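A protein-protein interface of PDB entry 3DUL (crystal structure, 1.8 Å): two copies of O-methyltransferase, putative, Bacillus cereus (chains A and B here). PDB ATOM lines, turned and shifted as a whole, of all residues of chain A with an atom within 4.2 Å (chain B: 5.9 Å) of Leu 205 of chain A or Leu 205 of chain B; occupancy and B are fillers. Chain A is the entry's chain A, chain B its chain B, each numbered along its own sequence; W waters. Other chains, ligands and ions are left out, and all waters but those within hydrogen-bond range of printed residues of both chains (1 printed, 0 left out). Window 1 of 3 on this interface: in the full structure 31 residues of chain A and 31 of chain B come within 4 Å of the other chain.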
ATOM      1  N   PHE A  49     -16.754   4.325  -1.160  1.00  0.00           N
ATOM      2  CA  PHE A  49     -16.665   3.170  -2.050  1.00  0.00           C
ATOM      3  C   PHE A  49     -17.191   1.946  -1.311  1.00  0.00           C
ATOM      4  O   PHE A  49     -17.981   1.162  -1.841  1.00  0.00           O
ATOM      5  CB  PHE A  49     -15.218   2.932  -2.447  1.00  0.00           C
ATOM      6  CG  PHE A  49     -14.996   1.639  -3.178  1.00  0.00           C
ATOM      7  CD1 PHE A  49     -15.273   1.532  -4.532  1.00  0.00           C
ATOM      8  CD2 PHE A  49     -14.507   0.525  -2.499  1.00  0.00           C
ATOM      9  CE1 PHE A  49     -15.064   0.335  -5.213  1.00  0.00           C
ATOM     10  CE2 PHE A  49     -14.295  -0.680  -3.169  1.00  0.00           C
ATOM     11  CZ  PHE A  49     -14.574  -0.772  -4.530  1.00  0.00           C
ATOM     12  N   ALA A 204      -7.141  -4.543  -8.951  1.00  0.00           N
ATOM     13  CA  ALA A 204      -6.555  -3.609  -8.008  1.00  0.00           C
ATOM     14  C   ALA A 204      -6.829  -2.183  -8.440  1.00  0.00           C
ATOM     15  O   ALA A 204      -6.833  -1.867  -9.629  1.00  0.00           O
ATOM     16  CB  ALA A 204      -5.059  -3.836  -7.903  1.00  0.00           C
ATOM     17  N   LEU A 205      -7.075  -1.323  -7.463  1.00  0.00           N
ATOM     18  CA  LEU A 205      -7.315   0.081  -7.744  1.00  0.00           C
ATOM     19  C   LEU A 205      -6.922   0.896  -6.530  1.00  0.00           C
ATOM     20  O   LEU A 205      -6.349   0.374  -5.574  1.00  0.00           O
ATOM     21  CB  LEU A 205      -8.790   0.332  -8.083  1.00  0.00           C
ATOM     22  CG  LEU A 205      -9.871  -0.023  -7.062  1.00  0.00           C
ATOM     23  CD1 LEU A 205     -11.123   0.812  -7.328  1.00  0.00           C
ATOM     24  CD2 LEU A 205     -10.199  -1.496  -7.156  1.00  0.00           C
ATOM     25  N   GLN A 206      -7.207   2.186  -6.577  1.00  0.00           N
ATOM     26  CA  GLN A 206      -6.897   3.042  -5.451  1.00  0.00           C
ATOM     27  C   GLN A 206      -7.812   4.242  -5.430  1.00  0.00           C
ATOM     28  O   GLN A 206      -8.605   4.460  -6.354  1.00  0.00           O
ATOM     29  CB  GLN A 206      -5.433   3.483  -5.477  1.00  0.00           C
ATOM     30  CG  GLN A 206      -4.905   3.868  -6.832  1.00  0.00           C
ATOM     31  CD  GLN A 206      -4.222   2.718  -7.550  1.00  0.00           C
ATOM     32  OE1 GLN A 206      -4.012   2.770  -8.756  1.00  0.00           O
ATOM     33  NE2 GLN A 206      -3.863   1.680  -6.806  1.00  0.00           N
ATOM     34  N   ASP A 214      -4.609   5.387  -1.441  1.00  0.00           N
ATOM     35  CA  ASP A 214      -4.807   4.092  -0.806  1.00  0.00           C
ATOM     36  C   ASP A 214      -4.990   3.023  -1.866  1.00  0.00           C
ATOM     37  O   ASP A 214      -5.963   3.050  -2.612  1.00  0.00           O
ATOM     38  CB  ASP A 214      -6.054   4.109   0.080  1.00  0.00           C
ATOM     39  CG  ASP A 214      -5.849   4.881   1.360  1.00  0.00           C
ATOM     40  OD1 ASP A 214      -5.540   6.090   1.287  1.00  0.00           O
ATOM     41  OD2 ASP A 214      -6.000   4.273   2.443  1.00  0.00           O
ATOM     42  N   GLY A 215      -4.057   2.082  -1.924  1.00  0.00           N
ATOM     43  CA  GLY A 215      -4.159   1.010  -2.896  1.00  0.00           C
ATOM     44  C   GLY A 215      -4.856  -0.183  -2.277  1.00  0.00           C
ATOM     45  O   GLY A 215      -4.591  -0.526  -1.127  1.00  0.00           O
ATOM     46  N   PHE A 216      -5.758  -0.813  -3.021  1.00  0.00           N
ATOM     47  CA  PHE A 216      -6.457  -1.976  -2.493  1.00  0.00           C
ATOM     48  C   PHE A 216      -6.916  -2.964  -3.551  1.00  0.00           C
ATOM     49  O   PHE A 216      -7.128  -2.613  -4.709  1.00  0.00           O
ATOM     50  CB  PHE A 216      -7.661  -1.552  -1.641  1.00  0.00           C
ATOM     51  CG  PHE A 216      -8.656  -0.690  -2.364  1.00  0.00           C
ATOM     52  CD1 PHE A 216      -8.469   0.685  -2.457  1.00  0.00           C
ATOM     53  CD2 PHE A 216      -9.787  -1.248  -2.940  1.00  0.00           C
ATOM     54  CE1 PHE A 216      -9.401   1.493  -3.113  1.00  0.00           C
ATOM     55  CE2 PHE A 216     -10.724  -0.453  -3.598  1.00  0.00           C
ATOM     56  CZ  PHE A 216     -10.528   0.925  -3.682  1.00  0.00           C
ATOM     57  N   MET A 218      -9.718  -5.728  -4.970  1.00  0.00           N
ATOM     58  CA  MET A 218     -11.145  -5.987  -4.910  1.00  0.00           C
ATOM     59  C   MET A 218     -11.286  -7.365  -5.526  1.00  0.00           C
ATOM     60  O   MET A 218     -10.929  -7.573  -6.688  1.00  0.00           O
ATOM     61  CB  MET A 218     -11.948  -4.965  -5.719  1.00  0.00           C
ATOM     62  CG  MET A 218     -13.413  -5.357  -5.863  1.00  0.00           C
ATOM     63  SD  MET A 218     -14.519  -4.077  -6.815  1.00  0.00           S
ATOM     64  CE  MET A 218     -16.229  -4.617  -6.157  1.00  0.00           C
ATOM     65  N   PHE B  49     -12.476  -4.618 -13.242  1.00  0.00           N
ATOM     66  CA  PHE B  49     -13.345  -3.902 -12.312  1.00  0.00           C
ATOM     67  C   PHE B  49     -14.752  -3.847 -12.883  1.00  0.00           C
ATOM     68  O   PHE B  49     -15.742  -4.088 -12.189  1.00  0.00           O
ATOM     69  CB  PHE B  49     -12.828  -2.477 -12.103  1.00  0.00           C
ATOM     70  CG  PHE B  49     -13.757  -1.608 -11.307  1.00  0.00           C
ATOM     71  CD1 PHE B  49     -13.756  -1.647  -9.918  1.00  0.00           C
ATOM     72  CD2 PHE B  49     -14.643  -0.750 -11.952  1.00  0.00           C
ATOM     73  CE1 PHE B  49     -14.625  -0.841  -9.178  1.00  0.00           C
ATOM     74  CE2 PHE B  49     -15.515   0.057 -11.222  1.00  0.00           C
ATOM     75  CZ  PHE B  49     -15.502   0.009  -9.830  1.00  0.00           C
ATOM     76  N   ARG B 170      -4.054   9.886 -15.891  1.00  0.00           N
ATOM     77  CA  ARG B 170      -2.964  10.542 -15.171  1.00  0.00           C
ATOM     78  C   ARG B 170      -1.619   9.915 -15.507  1.00  0.00           C
ATOM     79  O   ARG B 170      -1.105   9.094 -14.744  1.00  0.00           O
ATOM     80  CB  ARG B 170      -3.170  10.436 -13.656  1.00  0.00           C
ATOM     81  CG  ARG B 170      -4.395  11.137 -13.102  1.00  0.00           C
ATOM     82  CD  ARG B 170      -4.600  10.772 -11.623  1.00  0.00           C
ATOM     83  NE  ARG B 170      -5.808  11.375 -11.059  1.00  0.00           N
ATOM     84  CZ  ARG B 170      -7.000  11.326 -11.642  1.00  0.00           C
ATOM     85  NH1 ARG B 170      -7.136  10.700 -12.802  1.00  0.00           N
ATOM     86  NH2 ARG B 170      -8.050  11.904 -11.074  1.00  0.00           N
ATOM     87  N   TYR B 191     -17.228  17.131 -11.505  1.00  0.00           N
ATOM     88  CA  TYR B 191     -17.512  16.499 -10.221  1.00  0.00           C
ATOM     89  C   TYR B 191     -18.409  17.424  -9.409  1.00  0.00           C
ATOM     90  O   TYR B 191     -19.137  16.979  -8.520  1.00  0.00           O
ATOM     91  CB  TYR B 191     -16.216  16.212  -9.468  1.00  0.00           C
ATOM     92  CG  TYR B 191     -15.430  15.053 -10.044  1.00  0.00           C
ATOM     93  CD1 TYR B 191     -15.929  13.752  -9.987  1.00  0.00           C
ATOM     94  CD2 TYR B 191     -14.192  15.255 -10.649  1.00  0.00           C
ATOM     95  CE1 TYR B 191     -15.213  12.681 -10.517  1.00  0.00           C
ATOM     96  CE2 TYR B 191     -13.466  14.189 -11.182  1.00  0.00           C
ATOM     97  CZ  TYR B 191     -13.984  12.907 -11.111  1.00  0.00           C
ATOM     98  OH  TYR B 191     -13.272  11.856 -11.641  1.00  0.00           O
ATOM     99  N   THR B 203     -18.508   8.319  -5.683  1.00  0.00           N
ATOM    100  CA  THR B 203     -17.149   8.403  -5.186  1.00  0.00           C
ATOM    101  C   THR B 203     -16.239   8.401  -6.414  1.00  0.00           C
ATOM    102  O   THR B 203     -16.705   8.195  -7.544  1.00  0.00           O
ATOM    103  CB  THR B 203     -16.782   7.218  -4.244  1.00  0.00           C
ATOM    104  OG1 THR B 203     -15.498   7.464  -3.664  1.00  0.00           O
ATOM    105  CG2 THR B 203     -16.738   5.902  -5.006  1.00  0.00           C
ATOM    106  N   ALA B 204     -14.957   8.659  -6.202  1.00  0.00           N
ATOM    107  CA  ALA B 204     -14.000   8.677  -7.301  1.00  0.00           C
ATOM    108  C   ALA B 204     -12.876   7.698  -7.018  1.00  0.00           C
ATOM    109  O   ALA B 204     -12.380   7.617  -5.894  1.00  0.00           O
ATOM    110  CB  ALA B 204     -13.443  10.079  -7.492  1.00  0.00           C
ATOM    111  N   LEU B 205     -12.470   6.967  -8.052  1.00  0.00           N
ATOM    112  CA  LEU B 205     -11.417   5.967  -7.939  1.00  0.00           C
ATOM    113  C   LEU B 205     -10.448   6.088  -9.110  1.00  0.00           C
ATOM    114  O   LEU B 205     -10.676   6.855 -10.038  1.00  0.00           O
ATOM    115  CB  LEU B 205     -12.031   4.567  -7.988  1.00  0.00           C
ATOM    116  CG  LEU B 205     -13.339   4.407  -7.225  1.00  0.00           C
ATOM    117  CD1 LEU B 205     -14.163   3.283  -7.832  1.00  0.00           C
ATOM    118  CD2 LEU B 205     -13.021   4.159  -5.761  1.00  0.00           C
ATOM    119  N   GLN B 206      -9.374   5.315  -9.056  1.00  0.00           N
ATOM    120  CA  GLN B 206      -8.397   5.295 -10.135  1.00  0.00           C
ATOM    121  C   GLN B 206      -7.860   3.871 -10.222  1.00  0.00           C
ATOM    122  O   GLN B 206      -7.929   3.106  -9.255  1.00  0.00           O
ATOM    123  CB  GLN B 206      -7.247   6.269  -9.859  1.00  0.00           C
ATOM    124  CG  GLN B 206      -6.212   5.758  -8.869  1.00  0.00           C
ATOM    125  CD  GLN B 206      -5.049   6.723  -8.669  1.00  0.00           C
ATOM    126  OE1 GLN B 206      -4.054   6.394  -8.020  1.00  0.00           O
ATOM    127  NE2 GLN B 206      -5.175   7.923  -9.223  1.00  0.00           N
ATOM    128  N   THR B 207      -7.341   3.521 -11.389  1.00  0.00           N
ATOM    129  CA  THR B 207      -6.769   2.206 -11.617  1.00  0.00           C
ATOM    130  C   THR B 207      -5.631   2.452 -12.605  1.00  0.00           C
ATOM    131  O   THR B 207      -5.701   3.397 -13.391  1.00  0.00           O
ATOM    132  CB  THR B 207      -7.822   1.247 -12.215  1.00  0.00           C
ATOM    133  OG1 THR B 207      -7.327  -0.094 -12.174  1.00  0.00           O
ATOM    134  CG2 THR B 207      -8.139   1.626 -13.655  1.00  0.00           C
ATOM    135  N   VAL B 208      -4.581   1.636 -12.564  1.00  0.00           N
ATOM    136  CA  VAL B 208      -3.463   1.852 -13.480  1.00  0.00           C
ATOM    137  C   VAL B 208      -3.808   1.410 -14.891  1.00  0.00           C
ATOM    138  O   VAL B 208      -4.651   0.541 -15.088  1.00  0.00           O
ATOM    139  CB  VAL B 208      -2.184   1.102 -13.034  1.00  0.00           C
ATOM    140  CG1 VAL B 208      -2.319  -0.390 -13.296  1.00  0.00           C
ATOM    141  CG2 VAL B 208      -0.977   1.670 -13.766  1.00  0.00           C
ATOM    142  N   ASP B 214      -6.083   5.637 -14.820  1.00  0.00           N
ATOM    143  CA  ASP B 214      -7.414   5.998 -15.292  1.00  0.00           C
ATOM    144  C   ASP B 214      -8.233   6.520 -14.123  1.00  0.00           C
ATOM    145  O   ASP B 214      -8.459   5.800 -13.158  1.00  0.00           O
ATOM    146  CB  ASP B 214      -8.136   4.778 -15.863  1.00  0.00           C
ATOM    147  CG  ASP B 214      -7.590   4.340 -17.202  1.00  0.00           C
ATOM    148  OD1 ASP B 214      -6.371   4.075 -17.298  1.00  0.00           O
ATOM    149  OD2 ASP B 214      -8.390   4.249 -18.157  1.00  0.00           O
ATOM    150  N   GLY B 215      -8.668   7.771 -14.204  1.00  0.00           N
ATOM    151  CA  GLY B 215      -9.483   8.325 -13.139  1.00  0.00           C
ATOM    152  C   GLY B 215     -10.942   8.146 -13.504  1.00  0.00           C
ATOM    153  O   GLY B 215     -11.320   8.374 -14.654  1.00  0.00           O
ATOM    154  N   PHE B 216     -11.776   7.716 -12.559  1.00  0.00           N
ATOM    155  CA  PHE B 216     -13.191   7.554 -12.870  1.00  0.00           C
ATOM    156  C   PHE B 216     -14.126   7.698 -11.679  1.00  0.00           C
ATOM    157  O   PHE B 216     -13.723   7.556 -10.530  1.00  0.00           O
ATOM    158  CB  PHE B 216     -13.454   6.209 -13.566  1.00  0.00           C
ATOM    159  CG  PHE B 216     -13.077   5.002 -12.748  1.00  0.00           C
ATOM    160  CD1 PHE B 216     -11.763   4.550 -12.707  1.00  0.00           C
ATOM    161  CD2 PHE B 216     -14.043   4.307 -12.035  1.00  0.00           C
ATOM    162  CE1 PHE B 216     -11.412   3.417 -11.966  1.00  0.00           C
ATOM    163  CE2 PHE B 216     -13.705   3.170 -11.288  1.00  0.00           C
ATOM    164  CZ  PHE B 216     -12.389   2.726 -11.255  1.00  0.00           C
ATOM    165  N   ILE B 217     -15.381   8.003 -11.976  1.00  0.00           N
ATOM    166  CA  ILE B 217     -16.395   8.161 -10.941  1.00  0.00           C
ATOM    167  C   ILE B 217     -17.258   6.906 -10.902  1.00  0.00           C
ATOM    168  O   ILE B 217     -17.505   6.274 -11.923  1.00  0.00           O
ATOM    169  CB  ILE B 217     -17.329   9.360 -11.230  1.00  0.00           C
ATOM    170  CG1 ILE B 217     -18.356   9.508 -10.104  1.00  0.00           C
ATOM    171  CG2 ILE B 217     -18.055   9.150 -12.546  1.00  0.00           C
ATOM    172  CD1 ILE B 217     -19.473  10.486 -10.402  1.00  0.00           C
ATOM    173  N   MET B 218     -17.686   6.528  -9.704  1.00  0.00           N
ATOM    174  CA  MET B 218     -18.569   5.392  -9.556  1.00  0.00           C
ATOM    175  C   MET B 218     -19.764   5.989  -8.825  1.00  0.00           C
ATOM    176  O   MET B 218     -19.607   6.533  -7.734  1.00  0.00           O
ATOM    177  CB  MET B 218     -17.942   4.291  -8.695  1.00  0.00           C
ATOM    178  CG  MET B 218     -18.896   3.145  -8.452  1.00  0.00           C
ATOM    179  SD  MET B 218     -18.158   1.735  -7.349  1.00  0.00           S
ATOM    180  CE  MET B 218     -18.841   2.310  -5.616  1.00  0.00           C
HETATM  181  O   HOH W   1      -4.647  -0.809 -10.744  1.00  0.00           O
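O of Ala 204 of chain A is in hydrogen-bond range of OG1 of Thr 207 of chain B (3.1 Å). The backbone NH of Gln 206 of chain A sits at hydrogen-bond distance from the backbone carbonyl oxygen of Gln 206 of chain B, at 2.9 Å.
The backbone carbonyl oxygen (O) of Leu 205 of chain A is in hydrogen-bond range of the backbone NH (N) of Phe 216 of chain A (2.9 Å). The backbone NH of Met 218 of chain B lies within hydrogen-bond range of the backbone carbonyl oxygen of Thr 203 of chain B, at 2.9 Å. N of Leu 205 of chain B sits at hydrogen-bond distance from O of Phe 216 of chain B (2.8 Å). The backbone NH (N) of Asp 214 of chain B lies within hydrogen-bond range of the backbone carbonyl oxygen (O) of Thr 207 of chain B.
Among the printed residues, merely in contact across the chains: Leu 205 of chain A with Gln 206 of chain B (3.1 Å), Gln 206 of chain A with Leu 205 of chain B (3.6 Å), Phe 49 of chain A with Leu 205 of chain B (3.7 Å), Phe 49 of chain A with Met 218 of chain B (3.8 Å) and Leu 205 of chain A with Leu 205 of chain B (3.9 Å).
Printed residues of chain B within 4 Å of Ala 204 of chain A: Thr 207. Of chain B, only Leu 205 (3.9 Å) and Gln 206 (3.1 Å) come within 4 Å of Leu 205 of chain A. Of the printed residues of chain B, Gln 206 of chain A touches Leu 205 (3.6 Å) and Gln 206 (2.9 Å). Of chain A, only Phe 49 (3.7 Å), Leu 205 (3.9 Å) and Gln 206 (3.6 Å) come within 4 Å of Leu 205 of chain B. Phe 216 of chain B touches none of the printed residues of chain A. Printed residues of chain A within 4 Å of Met 218 of chain B: Phe 49. The nearest residue of chain B that does not touch Leu 205 of chain A is Phe 49 of chain B (4.3 Å).
Hydrophobic or aromatic side chains of chain A within 4 Å of the printed part of chain B: Phe 49 and Leu 205.
Phe 49 of chain A touches Leu 205 of chain B, but with the chains exchanged Leu 205 of chain A does not touch Phe 49 of chain B (4.3 Å). Phe 49 of chain A touches Met 218 of chain B, but with the chains exchanged Met 218 of chain A does not touch Phe 49 of chain B (4.01 Å). Leu 205 of chain B touches its own counterpart, Leu 205 of chain A. Leu 205 of chain A touches Gln 206 of chain B, and with the chains exchanged Gln 206 of chain A touches Leu 205 of chain B.
Water W1 lies within hydrogen-bond range of O of Ala 204 of chain A (2.7 Å), N of Val 208 of chain B (3.0 Å) and OG1 of Thr 207 of chain B (3.1 Å).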
